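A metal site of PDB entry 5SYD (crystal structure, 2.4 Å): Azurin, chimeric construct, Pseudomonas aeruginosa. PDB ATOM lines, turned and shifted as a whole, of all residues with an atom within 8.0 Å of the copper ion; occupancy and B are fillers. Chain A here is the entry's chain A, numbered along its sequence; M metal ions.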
ATOM      1  N   MET A   4      10.802  33.890  -9.236  1.00  0.00           N
ATOM      2  CA  MET A   4      10.161  32.751  -8.602  1.00  0.00           C
ATOM      3  C   MET A   4      11.132  32.138  -7.603  1.00  0.00           C
ATOM      4  O   MET A   4      12.241  31.752  -7.981  1.00  0.00           O
ATOM      5  CB  MET A   4       9.758  31.722  -9.647  1.00  0.00           C
ATOM      6  CG  MET A   4       8.898  30.596  -9.114  1.00  0.00           C
ATOM      7  SD  MET A   4       7.487  31.094  -8.130  1.00  0.00           S
ATOM      8  CE  MET A   4       6.472  29.664  -8.446  1.00  0.00           C
ATOM      9  N   GLY A   5      10.705  32.032  -6.350  1.00  0.00           N
ATOM     10  CA  GLY A   5      11.515  31.364  -5.341  1.00  0.00           C
ATOM     11  C   GLY A   5      10.676  30.809  -4.197  1.00  0.00           C
ATOM     12  O   GLY A   5       9.567  31.272  -3.925  1.00  0.00           O
ATOM     13  N   HIS A   6      11.222  29.779  -3.561  1.00  0.00           N
ATOM     14  CA  HIS A   6      10.661  29.237  -2.344  1.00  0.00           C
ATOM     15  C   HIS A   6      11.759  29.135  -1.304  1.00  0.00           C
ATOM     16  O   HIS A   6      12.940  28.973  -1.647  1.00  0.00           O
ATOM     17  CB  HIS A   6      10.014  27.843  -2.548  1.00  0.00           C
ATOM     18  CG  HIS A   6       9.011  27.787  -3.660  1.00  0.00           C
ATOM     19  ND1 HIS A   6       7.850  28.530  -3.669  1.00  0.00           N
ATOM     20  CD2 HIS A   6       8.981  27.052  -4.801  1.00  0.00           C
ATOM     21  CE1 HIS A   6       7.168  28.274  -4.765  1.00  0.00           C
ATOM     22  NE2 HIS A   6       7.832  27.370  -5.465  1.00  0.00           N
ATOM     23  N   ASN A   7      11.380  29.258  -0.038  1.00  0.00           N
ATOM     24  CA  ASN A   7      12.264  28.938   1.076  1.00  0.00           C
ATOM     25  C   ASN A   7      11.436  28.180   2.103  1.00  0.00           C
ATOM     26  O   ASN A   7      10.237  27.942   1.929  1.00  0.00           O
ATOM     27  CB  ASN A   7      12.947  30.184   1.652  1.00  0.00           C
ATOM     28  CG  ASN A   7      11.959  31.217   2.188  1.00  0.00           C
ATOM     29  OD1 ASN A   7      10.770  30.967   2.304  1.00  0.00           O
ATOM     30  ND2 ASN A   7      12.485  32.395   2.515  1.00  0.00           N
ATOM     31  N   TRP A   8      12.092  27.768   3.176  1.00  0.00           N
ATOM     32  CA  TRP A   8      11.433  27.014   4.237  1.00  0.00           C
ATOM     33  C   TRP A   8      11.836  27.633   5.559  1.00  0.00           C
ATOM     34  O   TRP A   8      13.011  27.582   5.945  1.00  0.00           O
ATOM     35  CB  TRP A   8      11.806  25.525   4.172  1.00  0.00           C
ATOM     36  CG  TRP A   8      11.032  24.682   5.131  1.00  0.00           C
ATOM     37  CD1 TRP A   8       9.861  24.032   4.884  1.00  0.00           C
ATOM     38  CD2 TRP A   8      11.369  24.416   6.497  1.00  0.00           C
ATOM     39  NE1 TRP A   8       9.446  23.361   6.012  1.00  0.00           N
ATOM     40  CE2 TRP A   8      10.351  23.576   7.013  1.00  0.00           C
ATOM     41  CE3 TRP A   8      12.425  24.782   7.328  1.00  0.00           C
ATOM     42  CZ2 TRP A   8      10.369  23.116   8.328  1.00  0.00           C
ATOM     43  CZ3 TRP A   8      12.438  24.328   8.637  1.00  0.00           C
ATOM     44  CH2 TRP A   8      11.422  23.504   9.119  1.00  0.00           C
ATOM     45  N   LEU A  46      16.658  31.010  -0.078  1.00  0.00           N
ATOM     46  CA  LEU A  46      15.703  31.082  -1.169  1.00  0.00           C
ATOM     47  C   LEU A  46      16.291  30.379  -2.380  1.00  0.00           C
ATOM     48  O   LEU A  46      17.432  30.639  -2.770  1.00  0.00           O
ATOM     49  CB  LEU A  46      15.406  32.551  -1.522  1.00  0.00           C
ATOM     50  CG  LEU A  46      14.118  32.908  -2.269  1.00  0.00           C
ATOM     51  CD1 LEU A  46      12.863  32.604  -1.450  1.00  0.00           C
ATOM     52  CD2 LEU A  46      14.167  34.367  -2.702  1.00  0.00           C
ATOM     53  N   ILE A  47      15.523  29.466  -2.979  1.00  0.00           N
ATOM     54  CA  ILE A  47      16.017  28.675  -4.093  1.00  0.00           C
ATOM     55  C   ILE A  47      15.100  28.857  -5.278  1.00  0.00           C
ATOM     56  O   ILE A  47      13.876  28.969  -5.125  1.00  0.00           O
ATOM     57  CB  ILE A  47      16.178  27.185  -3.721  1.00  0.00           C
ATOM     58  CG1 ILE A  47      14.832  26.580  -3.308  1.00  0.00           C
ATOM     59  CG2 ILE A  47      17.228  27.007  -2.627  1.00  0.00           C
ATOM     60  CD1 ILE A  47      14.900  25.089  -3.061  1.00  0.00           C
ATOM     61  N   PHE A  71       6.680  27.706   6.689  1.00  0.00           N
ATOM     62  CA  PHE A  71       6.067  28.506   5.642  1.00  0.00           C
ATOM     63  C   PHE A  71       7.152  29.076   4.737  1.00  0.00           C
ATOM     64  O   PHE A  71       8.330  29.150   5.117  1.00  0.00           O
ATOM     65  CB  PHE A  71       5.223  29.640   6.251  1.00  0.00           C
ATOM     66  CG  PHE A  71       5.952  30.418   7.326  1.00  0.00           C
ATOM     67  CD1 PHE A  71       5.819  30.055   8.661  1.00  0.00           C
ATOM     68  CD2 PHE A  71       6.778  31.475   7.010  1.00  0.00           C
ATOM     69  CE1 PHE A  71       6.487  30.745   9.652  1.00  0.00           C
ATOM     70  CE2 PHE A  71       7.449  32.174   7.990  1.00  0.00           C
ATOM     71  CZ  PHE A  71       7.308  31.799   9.323  1.00  0.00           C
ATOM     72  N   CYS A  72       6.730  29.513   3.553  1.00  0.00           N
ATOM     73  CA  CYS A  72       7.584  30.275   2.661  1.00  0.00           C
ATOM     74  C   CYS A  72       7.296  31.770   2.814  1.00  0.00           C
ATOM     75  O   CYS A  72       6.139  32.182   2.883  1.00  0.00           O
ATOM     76  CB  CYS A  72       7.375  29.857   1.206  1.00  0.00           C
ATOM     77  SG  CYS A  72       8.381  30.833   0.103  1.00  0.00           S
ATOM     78  N   THR A  73       8.354  32.572   2.834  1.00  0.00           N
ATOM     79  CA  THR A  73       8.227  34.012   3.027  1.00  0.00           C
ATOM     80  C   THR A  73       8.253  34.785   1.718  1.00  0.00           C
ATOM     81  O   THR A  73       8.095  36.012   1.744  1.00  0.00           O
ATOM     82  CB  THR A  73       9.330  34.530   3.945  1.00  0.00           C
ATOM     83  OG1 THR A  73      10.609  34.304   3.344  1.00  0.00           O
ATOM     84  CG2 THR A  73       9.268  33.820   5.287  1.00  0.00           C
ATOM     85  N   PHE A  74       8.430  34.109   0.594  1.00  0.00           N
ATOM     86  CA  PHE A  74       8.367  34.788  -0.686  1.00  0.00           C
ATOM     87  C   PHE A  74       7.035  35.526  -0.788  1.00  0.00           C
ATOM     88  O   PHE A  74       5.982  34.918  -0.512  1.00  0.00           O
ATOM     89  CB  PHE A  74       8.520  33.778  -1.822  1.00  0.00           C
ATOM     90  CG  PHE A  74       8.779  34.382  -3.170  1.00  0.00           C
ATOM     91  CD1 PHE A  74       7.736  34.701  -4.014  1.00  0.00           C
ATOM     92  CD2 PHE A  74      10.082  34.614  -3.596  1.00  0.00           C
ATOM     93  CE1 PHE A  74       7.971  35.248  -5.266  1.00  0.00           C
ATOM     94  CE2 PHE A  74      10.330  35.159  -4.845  1.00  0.00           C
ATOM     95  CZ  PHE A  74       9.275  35.472  -5.668  1.00  0.00           C
ATOM     96  N   PRO A  75       7.022  36.818  -1.154  1.00  0.00           N
ATOM     97  CA  PRO A  75       5.801  37.627  -1.026  1.00  0.00           C
ATOM     98  C   PRO A  75       4.564  36.972  -1.624  1.00  0.00           C
ATOM     99  O   PRO A  75       4.549  36.599  -2.800  1.00  0.00           O
ATOM    100  CB  PRO A  75       6.167  38.916  -1.755  1.00  0.00           C
ATOM    101  CG  PRO A  75       7.660  39.020  -1.611  1.00  0.00           C
ATOM    102  CD  PRO A  75       8.162  37.596  -1.669  1.00  0.00           C
ATOM    103  N   GLY A  76       3.541  36.808  -0.788  1.00  0.00           N
ATOM    104  CA  GLY A  76       2.292  36.224  -1.192  1.00  0.00           C
ATOM    105  C   GLY A  76       2.220  34.718  -1.058  1.00  0.00           C
ATOM    106  O   GLY A  76       1.111  34.171  -0.947  1.00  0.00           O
ATOM    107  N   HIS A  77       3.362  34.037  -1.029  1.00  0.00           N
ATOM    108  CA  HIS A  77       3.362  32.571  -1.060  1.00  0.00           C
ATOM    109  C   HIS A  77       2.871  31.974   0.255  1.00  0.00           C
ATOM    110  O   HIS A  77       2.314  30.874   0.265  1.00  0.00           O
ATOM    111  CB  HIS A  77       4.763  32.065  -1.408  1.00  0.00           C
ATOM    112  CG  HIS A  77       5.129  32.276  -2.848  1.00  0.00           C
ATOM    113  ND1 HIS A  77       6.076  31.512  -3.497  1.00  0.00           N
ATOM    114  CD2 HIS A  77       4.661  33.148  -3.771  1.00  0.00           C
ATOM    115  CE1 HIS A  77       6.184  31.910  -4.752  1.00  0.00           C
ATOM    116  NE2 HIS A  77       5.341  32.901  -4.941  1.00  0.00           N
ATOM    117  N   SER A  78       3.074  32.676   1.379  1.00  0.00           N
ATOM    118  CA  SER A  78       2.707  32.141   2.689  1.00  0.00           C
ATOM    119  C   SER A  78       1.218  31.837   2.823  1.00  0.00           C
ATOM    120  O   SER A  78       0.828  31.177   3.786  1.00  0.00           O
ATOM    121  CB  SER A  78       3.145  33.116   3.783  1.00  0.00           C
ATOM    122  OG  SER A  78       2.724  34.430   3.481  1.00  0.00           O
ATOM    123  N   MET A  81       1.510  28.266   1.156  1.00  0.00           N
ATOM    124  CA  MET A  81       2.741  27.560   1.477  1.00  0.00           C
ATOM    125  C   MET A  81       3.036  27.684   2.970  1.00  0.00           C
ATOM    126  O   MET A  81       3.934  28.407   3.412  1.00  0.00           O
ATOM    127  CB  MET A  81       3.896  28.091   0.635  1.00  0.00           C
ATOM    128  CG  MET A  81       3.827  27.726  -0.829  1.00  0.00           C
ATOM    129  SD  MET A  81       5.303  28.313  -1.720  1.00  0.00           S
ATOM    130  CE  MET A  81       6.373  26.896  -1.471  1.00  0.00           C
ATOM    131  N   GLY A 102       8.488  22.625  -3.043  1.00  0.00           N
ATOM    132  CA  GLY A 102       7.597  23.695  -3.465  1.00  0.00           C
ATOM    133  C   GLY A 102       7.591  23.783  -4.976  1.00  0.00           C
ATOM    134  O   GLY A 102       8.657  23.764  -5.613  1.00  0.00           O
ATOM    135  N   ASN A 103       6.398  23.857  -5.559  1.00  0.00           N
ATOM    136  CA  ASN A 103       6.255  23.815  -7.003  1.00  0.00           C
ATOM    137  C   ASN A 103       5.811  25.189  -7.528  1.00  0.00           C
ATOM    138  O   ASN A 103       5.867  26.199  -6.813  1.00  0.00           O
ATOM    139  CB  ASN A 103       5.305  22.691  -7.426  1.00  0.00           C
ATOM    140  CG  ASN A 103       3.893  22.875  -6.919  1.00  0.00           C
ATOM    141  OD1 ASN A 103       3.581  23.832  -6.204  1.00  0.00           O
ATOM    142  ND2 ASN A 103       3.020  21.946  -7.275  1.00  0.00           N
ATOM    143  N   MET A 106       2.445  27.548  -5.907  1.00  0.00           N
ATOM    144  CA  MET A 106       2.441  28.028  -4.518  1.00  0.00           C
ATOM    145  C   MET A 106       2.024  26.916  -3.553  1.00  0.00           C
ATOM    146  O   MET A 106       1.223  27.134  -2.646  1.00  0.00           O
ATOM    147  CB  MET A 106       1.531  29.258  -4.345  1.00  0.00           C
ATOM    148  CG  MET A 106       1.996  30.505  -5.052  1.00  0.00           C
ATOM    149  SD  MET A 106       1.436  31.994  -4.214  1.00  0.00           S
ATOM    150  CE  MET A 106      -0.314  31.653  -4.063  1.00  0.00           C
ATOM    151  N   GLN A 107       2.579  25.724  -3.740  1.00  0.00           N
ATOM    152  CA  GLN A 107       2.229  24.580  -2.918  1.00  0.00           C
ATOM    153  C   GLN A 107       3.462  23.898  -2.365  1.00  0.00           C
ATOM    154  O   GLN A 107       4.430  23.645  -3.101  1.00  0.00           O
ATOM    155  CB  GLN A 107       1.404  23.559  -3.715  1.00  0.00           C
ATOM    156  CG  GLN A 107      -0.057  23.947  -3.939  1.00  0.00           C
ATOM    157  CD  GLN A 107      -0.888  23.889  -2.666  1.00  0.00           C
ATOM    158  OE1 GLN A 107      -1.929  24.522  -2.572  1.00  0.00           O
ATOM    159  NE2 GLN A 107      -0.425  23.108  -1.694  1.00  0.00           N
ATOM    160  N   PHE A 108       3.446  23.609  -1.065  1.00  0.00           N
ATOM    161  CA  PHE A 108       4.284  22.585  -0.483  1.00  0.00           C
ATOM    162  C   PHE A 108       3.607  21.232  -0.690  1.00  0.00           C
ATOM    163  O   PHE A 108       2.382  21.160  -0.813  1.00  0.00           O
ATOM    164  CB  PHE A 108       4.510  22.840   1.008  1.00  0.00           C
ATOM    165  CG  PHE A 108       5.575  23.853   1.320  1.00  0.00           C
ATOM    166  CD1 PHE A 108       6.780  23.850   0.641  1.00  0.00           C
ATOM    167  CD2 PHE A 108       5.379  24.806   2.305  1.00  0.00           C
ATOM    168  CE1 PHE A 108       7.772  24.776   0.942  1.00  0.00           C
ATOM    169  CE2 PHE A 108       6.357  25.734   2.604  1.00  0.00           C
ATOM    170  CZ  PHE A 108       7.562  25.723   1.919  1.00  0.00           C
ATOM    171  N   LEU A 126      14.830  20.915   1.195  1.00  0.00           N
ATOM    172  CA  LEU A 126      13.912  21.628   0.328  1.00  0.00           C
ATOM    173  C   LEU A 126      14.416  21.552  -1.110  1.00  0.00           C
ATOM    174  O   LEU A 126      15.597  21.784  -1.388  1.00  0.00           O
ATOM    175  CB  LEU A 126      13.788  23.092   0.753  1.00  0.00           C
ATOM    176  CG  LEU A 126      12.815  23.951  -0.071  1.00  0.00           C
ATOM    177  CD1 LEU A 126      11.362  23.546   0.228  1.00  0.00           C
ATOM    178  CD2 LEU A 126      13.029  25.433   0.181  1.00  0.00           C
ATOM    179  N   HIS A 128      13.017  22.583  -5.339  1.00  0.00           N
ATOM    180  CA  HIS A 128      12.157  23.459  -6.133  1.00  0.00           C
ATOM    181  C   HIS A 128      12.184  22.897  -7.548  1.00  0.00           C
ATOM    182  O   HIS A 128      12.914  23.397  -8.417  1.00  0.00           O
ATOM    183  CB  HIS A 128      12.641  24.914  -6.067  1.00  0.00           C
ATOM    184  CG  HIS A 128      11.754  25.902  -6.762  1.00  0.00           C
ATOM    185  ND1 HIS A 128      10.737  25.529  -7.616  1.00  0.00           N
ATOM    186  CD2 HIS A 128      11.759  27.254  -6.753  1.00  0.00           C
ATOM    187  CE1 HIS A 128      10.139  26.612  -8.086  1.00  0.00           C
ATOM    188  NE2 HIS A 128      10.753  27.674  -7.574  1.00  0.00           N
HETATM  189 CU    CU M   1       7.459  30.151  -2.089  1.00  0.00          CU
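A ring nitrogen (ND1) of His 6 sits close to the side-chain sulfur (SD) of Met 81. The backbone carbonyl oxygen of Asn 103 lies within hydrogen-bond range of a ring nitrogen (NE2) of His 6, at 2.7 Å. O of His 6 is in hydrogen-bond range of N of Ile 47 (2.9 Å). A ring nitrogen (ND1) of His 77 sits close to the side-chain sulfur (SD) of Met 81 (3.7 Å). The backbone NH of Cys 72 is in hydrogen-bond range of the backbone carbonyl oxygen of Met 81. SG of Cys 72 lies close to N of Phe 74, 3.3 Å away. The side-chain sulfur of Cys 72 sits close to the side-chain amide oxygen of Asn 7 (3.3 Å). The backbone carbonyl oxygen of Cys 72 lies close to the backbone NH of Ser 78, 3.4 Å away.
Gly 5 touches the copper ion. CB of Phe 74 touches the copper ion (3.8 Å). Within 4 Å of the copper ion: Gly 5, His 6, Cys 72, Phe 74, His 77 and Met 81.
ND1 of His 6 is bound to the copper ion, at 2.3 Å. The copper ion is bound by ND1 of His 77, 2.4 Å away. The side-chain sulfur (SG) of Cys 72 is bound to the copper ion, 2.5 Å away. The copper ion has three donor atoms within binding distance. Slightly farther from the copper ion lies the side-chain sulfur (SD) of Met 81 (2.9 Å).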
